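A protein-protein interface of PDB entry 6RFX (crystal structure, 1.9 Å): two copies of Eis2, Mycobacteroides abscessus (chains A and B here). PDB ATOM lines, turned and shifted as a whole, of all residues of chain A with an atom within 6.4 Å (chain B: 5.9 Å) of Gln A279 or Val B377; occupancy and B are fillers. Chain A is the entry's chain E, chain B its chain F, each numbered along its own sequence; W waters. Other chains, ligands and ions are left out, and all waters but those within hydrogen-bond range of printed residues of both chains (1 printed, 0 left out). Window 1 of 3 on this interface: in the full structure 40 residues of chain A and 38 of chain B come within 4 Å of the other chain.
The backbone carbonyl oxygen (O) of Pro A402 sits at hydrogen-bond distance from the side-chain hydroxyl (OG) of Ser B374, at 2.8 Å.
O of Gln B376 lies within hydrogen-bond range of OG of Ser B380, 3.2 Å away.
The side-chain amide oxygen (OE1) of Gln A279 sits at hydrogen-bond distance from the backbone NH (N) of Ala A404.
The side-chain hydroxyl of Ser B374 lies close to the backbone NH of Gln B376.
The backbone NH of Gln A279 is in hydrogen-bond range of the side-chain hydroxyl of Ser A277 (3.0 Å).
Gln A279 touches Val B377 (OE1 to CG2, 3.3 Å).
OE2 of Glu A281 touches CB of Ser B380 (3.6 Å).
Glu A281 touches Ala B381 (CB to CB, 3.9 Å).
Val B377 touches Tyr A284.
Tyr A284 touches Leu B378 (CD1 to CD2, 3.98 Å).
Gln B376 touches Pro A402.
Val B377 touches Pro A402 (CG2 to O, 3.997 Å).
Val A403 touches Gln B376 (CG2 to CG, 3.7 Å).
Ala A276 touches none of the printed residues of chain B.
Printed residues of chain B within 4 Å of Glu A281: Ser B380 and Ala B381.
Leu A282 touches none of the printed residues of chain B.
Printed residues of chain B within 4 Å of Tyr A284: Val B377 (3.8 Å) and Leu B378 (3.98 Å).
Of the printed residues of chain A, Val B377 touches Gln A279, Tyr A284 and Pro A402.
The nearest residue of chain B that does not touch Gln A279 is Ser B374 (4.1 Å).
The nearest printed residue of chain A that does not touch Ser B380 is Val A403 (5.4 Å).
Printed residues of chain A that touch a printed residue of chain B: Gln A279, Glu A281, Tyr A284, Pro A402 and Val A403.
Hydrophobic or aromatic side chains of chain A that line the printed part of chain B: Tyr A284, Pro A402 and Val A403.
Hydrophobic or aromatic side chains of chain B that line the printed part of chain A: Val B377, Leu B378 and Ala B381.
Among the printed residues, 9 pairs touch across the chains.
Among the printed residues, no Asp or Glu carboxylate lies within 4 Å of a Lys or Arg side-chain nitrogen of the other chain.
No position is printed for both chains.
Of the 9 pairs that touch across the chains among the printed residues, none has its exchanged pair printed and touching as well.
Water W1 lies within hydrogen-bond range of the side-chain hydroxyl of Tyr A284 (2.8 Å) and the backbone NH of Ser B374 (3.0 Å).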
ATOM      1  N   ALA A 136     -20.277 -15.595  26.011  1.00  0.00           N
ATOM      2  CA  ALA A 136     -21.625 -15.271  25.576  1.00  0.00           C
ATOM      3  C   ALA A 136     -22.423 -16.557  25.436  1.00  0.00           C
ATOM      4  O   ALA A 136     -21.926 -17.545  24.884  1.00  0.00           O
ATOM      5  CB  ALA A 136     -21.595 -14.533  24.236  1.00  0.00           C
ATOM      6  N   ALA A 276     -19.650 -19.378  24.375  1.00  0.00           N
ATOM      7  CA  ALA A 276     -19.119 -18.871  23.121  1.00  0.00           C
ATOM      8  C   ALA A 276     -18.319 -17.594  23.368  1.00  0.00           C
ATOM      9  O   ALA A 276     -18.321 -17.024  24.462  1.00  0.00           O
ATOM     10  CB  ALA A 276     -20.253 -18.596  22.134  1.00  0.00           C
ATOM     11  N   SER A 277     -17.621 -17.145  22.332  1.00  0.00           N
ATOM     12  CA  SER A 277     -16.938 -15.864  22.412  1.00  0.00           C
ATOM     13  C   SER A 277     -17.952 -14.733  22.303  1.00  0.00           C
ATOM     14  O   SER A 277     -18.962 -14.840  21.602  1.00  0.00           O
ATOM     15  CB  SER A 277     -15.913 -15.740  21.285  1.00  0.00           C
ATOM     16  OG  SER A 277     -15.393 -14.424  21.214  1.00  0.00           O
ATOM     17  N   VAL A 278     -17.681 -13.636  23.015  1.00  0.00           N
ATOM     18  CA  VAL A 278     -18.531 -12.455  22.889  1.00  0.00           C
ATOM     19  C   VAL A 278     -18.478 -11.904  21.471  1.00  0.00           C
ATOM     20  O   VAL A 278     -19.416 -11.238  21.018  1.00  0.00           O
ATOM     21  CB  VAL A 278     -18.164 -11.396  23.948  1.00  0.00           C
ATOM     22  CG1 VAL A 278     -18.337 -11.966  25.352  1.00  0.00           C
ATOM     23  CG2 VAL A 278     -16.744 -10.895  23.737  1.00  0.00           C
ATOM     24  N   GLN A 279     -17.390 -12.171  20.752  1.00  0.00           N
ATOM     25  CA  GLN A 279     -17.259 -11.844  19.336  1.00  0.00           C
ATOM     26  C   GLN A 279     -17.259 -13.108  18.480  1.00  0.00           C
ATOM     27  O   GLN A 279     -16.516 -13.215  17.503  1.00  0.00           O
ATOM     28  CB  GLN A 279     -16.004 -11.015  19.076  1.00  0.00           C
ATOM     29  CG  GLN A 279     -16.007  -9.648  19.737  1.00  0.00           C
ATOM     30  CD  GLN A 279     -14.702  -8.903  19.532  1.00  0.00           C
ATOM     31  OE1 GLN A 279     -13.779  -9.408  18.893  1.00  0.00           O
ATOM     32  NE2 GLN A 279     -14.619  -7.695  20.078  1.00  0.00           N
ATOM     33  N   GLU A 280     -18.088 -14.084  18.854  1.00  0.00           N
ATOM     34  CA  GLU A 280     -18.200 -15.317  18.086  1.00  0.00           C
ATOM     35  C   GLU A 280     -18.614 -14.999  16.656  1.00  0.00           C
ATOM     36  O   GLU A 280     -19.541 -14.218  16.427  1.00  0.00           O
ATOM     37  CB  GLU A 280     -19.247 -16.224  18.734  1.00  0.00           C
ATOM     38  CG  GLU A 280     -19.302 -17.626  18.158  1.00  0.00           C
ATOM     39  CD  GLU A 280     -18.071 -18.440  18.501  1.00  0.00           C
ATOM     40  OE1 GLU A 280     -17.640 -18.404  19.673  1.00  0.00           O
ATOM     41  OE2 GLU A 280     -17.528 -19.108  17.596  1.00  0.00           O
ATOM     42  N   GLU A 281     -17.918 -15.610  15.691  1.00  0.00           N
ATOM     43  CA  GLU A 281     -18.169 -15.299  14.285  1.00  0.00           C
ATOM     44  C   GLU A 281     -19.612 -15.586  13.885  1.00  0.00           C
ATOM     45  O   GLU A 281     -20.133 -14.957  12.956  1.00  0.00           O
ATOM     46  CB  GLU A 281     -17.200 -16.066  13.383  1.00  0.00           C
ATOM     47  CG  GLU A 281     -15.759 -15.572  13.425  1.00  0.00           C
ATOM     48  CD  GLU A 281     -14.945 -16.205  14.539  1.00  0.00           C
ATOM     49  OE1 GLU A 281     -15.536 -16.899  15.395  1.00  0.00           O
ATOM     50  OE2 GLU A 281     -13.710 -16.013  14.552  1.00  0.00           O
ATOM     51  N   LEU A 282     -20.270 -16.526  14.571  1.00  0.00           N
ATOM     52  CA  LEU A 282     -21.663 -16.838  14.266  1.00  0.00           C
ATOM     53  C   LEU A 282     -22.565 -15.621  14.422  1.00  0.00           C
ATOM     54  O   LEU A 282     -23.540 -15.472  13.675  1.00  0.00           O
ATOM     55  CB  LEU A 282     -22.148 -17.975  15.167  1.00  0.00           C
ATOM     56  CG  LEU A 282     -23.635 -18.335  15.087  1.00  0.00           C
ATOM     57  CD1 LEU A 282     -23.974 -18.936  13.732  1.00  0.00           C
ATOM     58  CD2 LEU A 282     -24.021 -19.280  16.213  1.00  0.00           C
ATOM     59  N   ARG A 283     -22.258 -14.739  15.378  1.00  0.00           N
ATOM     60  CA  ARG A 283     -23.087 -13.556  15.590  1.00  0.00           C
ATOM     61  C   ARG A 283     -23.124 -12.664  14.358  1.00  0.00           C
ATOM     62  O   ARG A 283     -24.106 -11.948  14.140  1.00  0.00           O
ATOM     63  CB  ARG A 283     -22.568 -12.754  16.781  1.00  0.00           C
ATOM     64  CG  ARG A 283     -22.442 -13.533  18.078  1.00  0.00           C
ATOM     65  CD  ARG A 283     -22.137 -12.575  19.212  1.00  0.00           C
ATOM     66  NE  ARG A 283     -23.164 -11.541  19.306  1.00  0.00           N
ATOM     67  CZ  ARG A 283     -22.988 -10.362  19.892  1.00  0.00           C
ATOM     68  NH1 ARG A 283     -21.817 -10.059  20.438  1.00  0.00           N
ATOM     69  NH2 ARG A 283     -23.982  -9.484  19.925  1.00  0.00           N
ATOM     70  N   TYR A 284     -22.067 -12.686  13.549  1.00  0.00           N
ATOM     71  CA  TYR A 284     -21.972 -11.829  12.376  1.00  0.00           C
ATOM     72  C   TYR A 284     -22.353 -12.538  11.084  1.00  0.00           C
ATOM     73  O   TYR A 284     -22.569 -11.868  10.070  1.00  0.00           O
ATOM     74  CB  TYR A 284     -20.562 -11.228  12.276  1.00  0.00           C
ATOM     75  CG  TYR A 284     -20.152 -10.558  13.565  1.00  0.00           C
ATOM     76  CD1 TYR A 284     -20.557  -9.261  13.854  1.00  0.00           C
ATOM     77  CD2 TYR A 284     -19.395 -11.235  14.513  1.00  0.00           C
ATOM     78  CE1 TYR A 284     -20.204  -8.650  15.041  1.00  0.00           C
ATOM     79  CE2 TYR A 284     -19.037 -10.632  15.703  1.00  0.00           C
ATOM     80  CZ  TYR A 284     -19.445  -9.340  15.961  1.00  0.00           C
ATOM     81  OH  TYR A 284     -19.090  -8.734  17.145  1.00  0.00           O
ATOM     82  N   TRP A 401      -6.981  -5.877  21.862  1.00  0.00           N
ATOM     83  CA  TRP A 401      -6.534  -6.786  20.816  1.00  0.00           C
ATOM     84  C   TRP A 401      -7.671  -6.959  19.826  1.00  0.00           C
ATOM     85  O   TRP A 401      -8.836  -6.986  20.246  1.00  0.00           O
ATOM     86  CB  TRP A 401      -6.137  -8.142  21.410  1.00  0.00           C
ATOM     87  CG  TRP A 401      -5.390  -9.024  20.459  1.00  0.00           C
ATOM     88  CD1 TRP A 401      -5.864 -10.136  19.829  1.00  0.00           C
ATOM     89  CD2 TRP A 401      -4.035  -8.860  20.017  1.00  0.00           C
ATOM     90  NE1 TRP A 401      -4.889 -10.680  19.028  1.00  0.00           N
ATOM     91  CE2 TRP A 401      -3.755  -9.914  19.126  1.00  0.00           C
ATOM     92  CE3 TRP A 401      -3.031  -7.925  20.292  1.00  0.00           C
ATOM     93  CZ2 TRP A 401      -2.514 -10.063  18.509  1.00  0.00           C
ATOM     94  CZ3 TRP A 401      -1.798  -8.074  19.677  1.00  0.00           C
ATOM     95  CH2 TRP A 401      -1.551  -9.134  18.796  1.00  0.00           C
ATOM     96  N   PRO A 402      -7.387  -7.072  18.525  1.00  0.00           N
ATOM     97  CA  PRO A 402      -8.476  -7.189  17.541  1.00  0.00           C
ATOM     98  C   PRO A 402      -9.344  -8.424  17.718  1.00  0.00           C
ATOM     99  O   PRO A 402     -10.479  -8.438  17.223  1.00  0.00           O
ATOM    100  CB  PRO A 402      -7.739  -7.208  16.194  1.00  0.00           C
ATOM    101  CG  PRO A 402      -6.407  -6.588  16.476  1.00  0.00           C
ATOM    102  CD  PRO A 402      -6.066  -6.980  17.880  1.00  0.00           C
ATOM    103  N   VAL A 403      -8.853  -9.458  18.394  1.00  0.00           N
ATOM    104  CA  VAL A 403      -9.620 -10.670  18.662  1.00  0.00           C
ATOM    105  C   VAL A 403      -9.902 -10.724  20.156  1.00  0.00           C
ATOM    106  O   VAL A 403      -8.972 -10.691  20.972  1.00  0.00           O
ATOM    107  CB  VAL A 403      -8.874 -11.929  18.195  1.00  0.00           C
ATOM    108  CG1 VAL A 403      -9.683 -13.175  18.526  1.00  0.00           C
ATOM    109  CG2 VAL A 403      -8.589 -11.855  16.703  1.00  0.00           C
ATOM    110  N   ALA A 404     -11.180 -10.804  20.513  1.00  0.00           N
ATOM    111  CA  ALA A 404     -11.550 -10.854  21.918  1.00  0.00           C
ATOM    112  C   ALA A 404     -11.050 -12.155  22.542  1.00  0.00           C
ATOM    113  O   ALA A 404     -11.046 -13.199  21.883  1.00  0.00           O
ATOM    114  CB  ALA A 404     -13.070 -10.774  22.064  1.00  0.00           C
ATOM    115  N   SER B 374     -15.485  -5.246  15.407  1.00  0.00           N
ATOM    116  CA  SER B 374     -14.087  -5.456  15.060  1.00  0.00           C
ATOM    117  C   SER B 374     -13.962  -5.848  13.592  1.00  0.00           C
ATOM    118  O   SER B 374     -14.656  -6.755  13.121  1.00  0.00           O
ATOM    119  CB  SER B 374     -13.479  -6.544  15.944  1.00  0.00           C
ATOM    120  OG  SER B 374     -12.118  -6.762  15.613  1.00  0.00           O
ATOM    121  N   LEU B 375     -13.074  -5.160  12.871  1.00  0.00           N
ATOM    122  CA  LEU B 375     -12.846  -5.498  11.470  1.00  0.00           C
ATOM    123  C   LEU B 375     -12.183  -6.861  11.324  1.00  0.00           C
ATOM    124  O   LEU B 375     -12.401  -7.551  10.322  1.00  0.00           O
ATOM    125  CB  LEU B 375     -12.003  -4.413  10.799  1.00  0.00           C
ATOM    126  CG  LEU B 375     -11.801  -4.525   9.286  1.00  0.00           C
ATOM    127  CD1 LEU B 375     -13.137  -4.452   8.559  1.00  0.00           C
ATOM    128  CD2 LEU B 375     -10.854  -3.444   8.785  1.00  0.00           C
ATOM    129  N   GLN B 376     -11.380  -7.267  12.312  1.00  0.00           N
ATOM    130  CA  GLN B 376     -10.717  -8.564  12.245  1.00  0.00           C
ATOM    131  C   GLN B 376     -11.722  -9.708  12.302  1.00  0.00           C
ATOM    132  O   GLN B 376     -11.584 -10.701  11.577  1.00  0.00           O
ATOM    133  CB  GLN B 376      -9.697  -8.686  13.377  1.00  0.00           C
ATOM    134  CG  GLN B 376      -9.038 -10.053  13.478  1.00  0.00           C
ATOM    135  CD  GLN B 376      -8.133 -10.356  12.300  1.00  0.00           C
ATOM    136  OE1 GLN B 376      -6.973  -9.948  12.276  1.00  0.00           O
ATOM    137  NE2 GLN B 376      -8.659 -11.076  11.317  1.00  0.00           N
ATOM    138  N   VAL B 377     -12.740  -9.590  13.157  1.00  0.00           N
ATOM    139  CA  VAL B 377     -13.728 -10.657  13.279  1.00  0.00           C
ATOM    140  C   VAL B 377     -14.571 -10.759  12.014  1.00  0.00           C
ATOM    141  O   VAL B 377     -14.943 -11.859  11.586  1.00  0.00           O
ATOM    142  CB  VAL B 377     -14.579 -10.473  14.547  1.00  0.00           C
ATOM    143  CG1 VAL B 377     -15.539 -11.643  14.719  1.00  0.00           C
ATOM    144  CG2 VAL B 377     -13.681 -10.336  15.767  1.00  0.00           C
ATOM    145  N   LEU B 378     -14.883  -9.619  11.390  1.00  0.00           N
ATOM    146  CA  LEU B 378     -15.576  -9.656  10.107  1.00  0.00           C
ATOM    147  C   LEU B 378     -14.744 -10.367   9.047  1.00  0.00           C
ATOM    148  O   LEU B 378     -15.296 -11.058   8.184  1.00  0.00           O
ATOM    149  CB  LEU B 378     -15.937  -8.240   9.654  1.00  0.00           C
ATOM    150  CG  LEU B 378     -16.904  -7.456  10.542  1.00  0.00           C
ATOM    151  CD1 LEU B 378     -17.284  -6.132   9.891  1.00  0.00           C
ATOM    152  CD2 LEU B 378     -18.148  -8.280  10.848  1.00  0.00           C
ATOM    153  N   ALA B 379     -13.417 -10.221   9.103  1.00  0.00           N
ATOM    154  CA  ALA B 379     -12.558 -10.957   8.183  1.00  0.00           C
ATOM    155  C   ALA B 379     -12.499 -12.434   8.550  1.00  0.00           C
ATOM    156  O   ALA B 379     -12.499 -13.298   7.665  1.00  0.00           O
ATOM    157  CB  ALA B 379     -11.156 -10.349   8.163  1.00  0.00           C
ATOM    158  N   SER B 380     -12.450 -12.743   9.850  1.00  0.00           N
ATOM    159  CA  SER B 380     -12.429 -14.137  10.284  1.00  0.00           C
ATOM    160  C   SER B 380     -13.672 -14.881   9.818  1.00  0.00           C
ATOM    161  O   SER B 380     -13.593 -16.051   9.425  1.00  0.00           O
ATOM    162  CB  SER B 380     -12.300 -14.212  11.807  1.00  0.00           C
ATOM    163  OG  SER B 380     -11.022 -13.778  12.236  1.00  0.00           O
ATOM    164  N   ALA B 381     -14.830 -14.219   9.850  1.00  0.00           N
ATOM    165  CA  ALA B 381     -16.074 -14.840   9.417  1.00  0.00           C
ATOM    166  C   ALA B 381     -16.213 -14.909   7.902  1.00  0.00           C
ATOM    167  O   ALA B 381     -17.150 -15.550   7.415  1.00  0.00           O
ATOM    168  CB  ALA B 381     -17.274 -14.104  10.018  1.00  0.00           C
ATOM    169  N   GLY B 382     -15.317 -14.271   7.150  1.00  0.00           N
ATOM    170  CA  GLY B 382     -15.364 -14.302   5.705  1.00  0.00           C
ATOM    171  C   GLY B 382     -16.139 -13.177   5.056  1.00  0.00           C
ATOM    172  O   GLY B 382     -16.261 -13.162   3.824  1.00  0.00           O
HETATM  173  O   HOH W   1     -16.786  -7.142  17.336  1.00  0.00           O
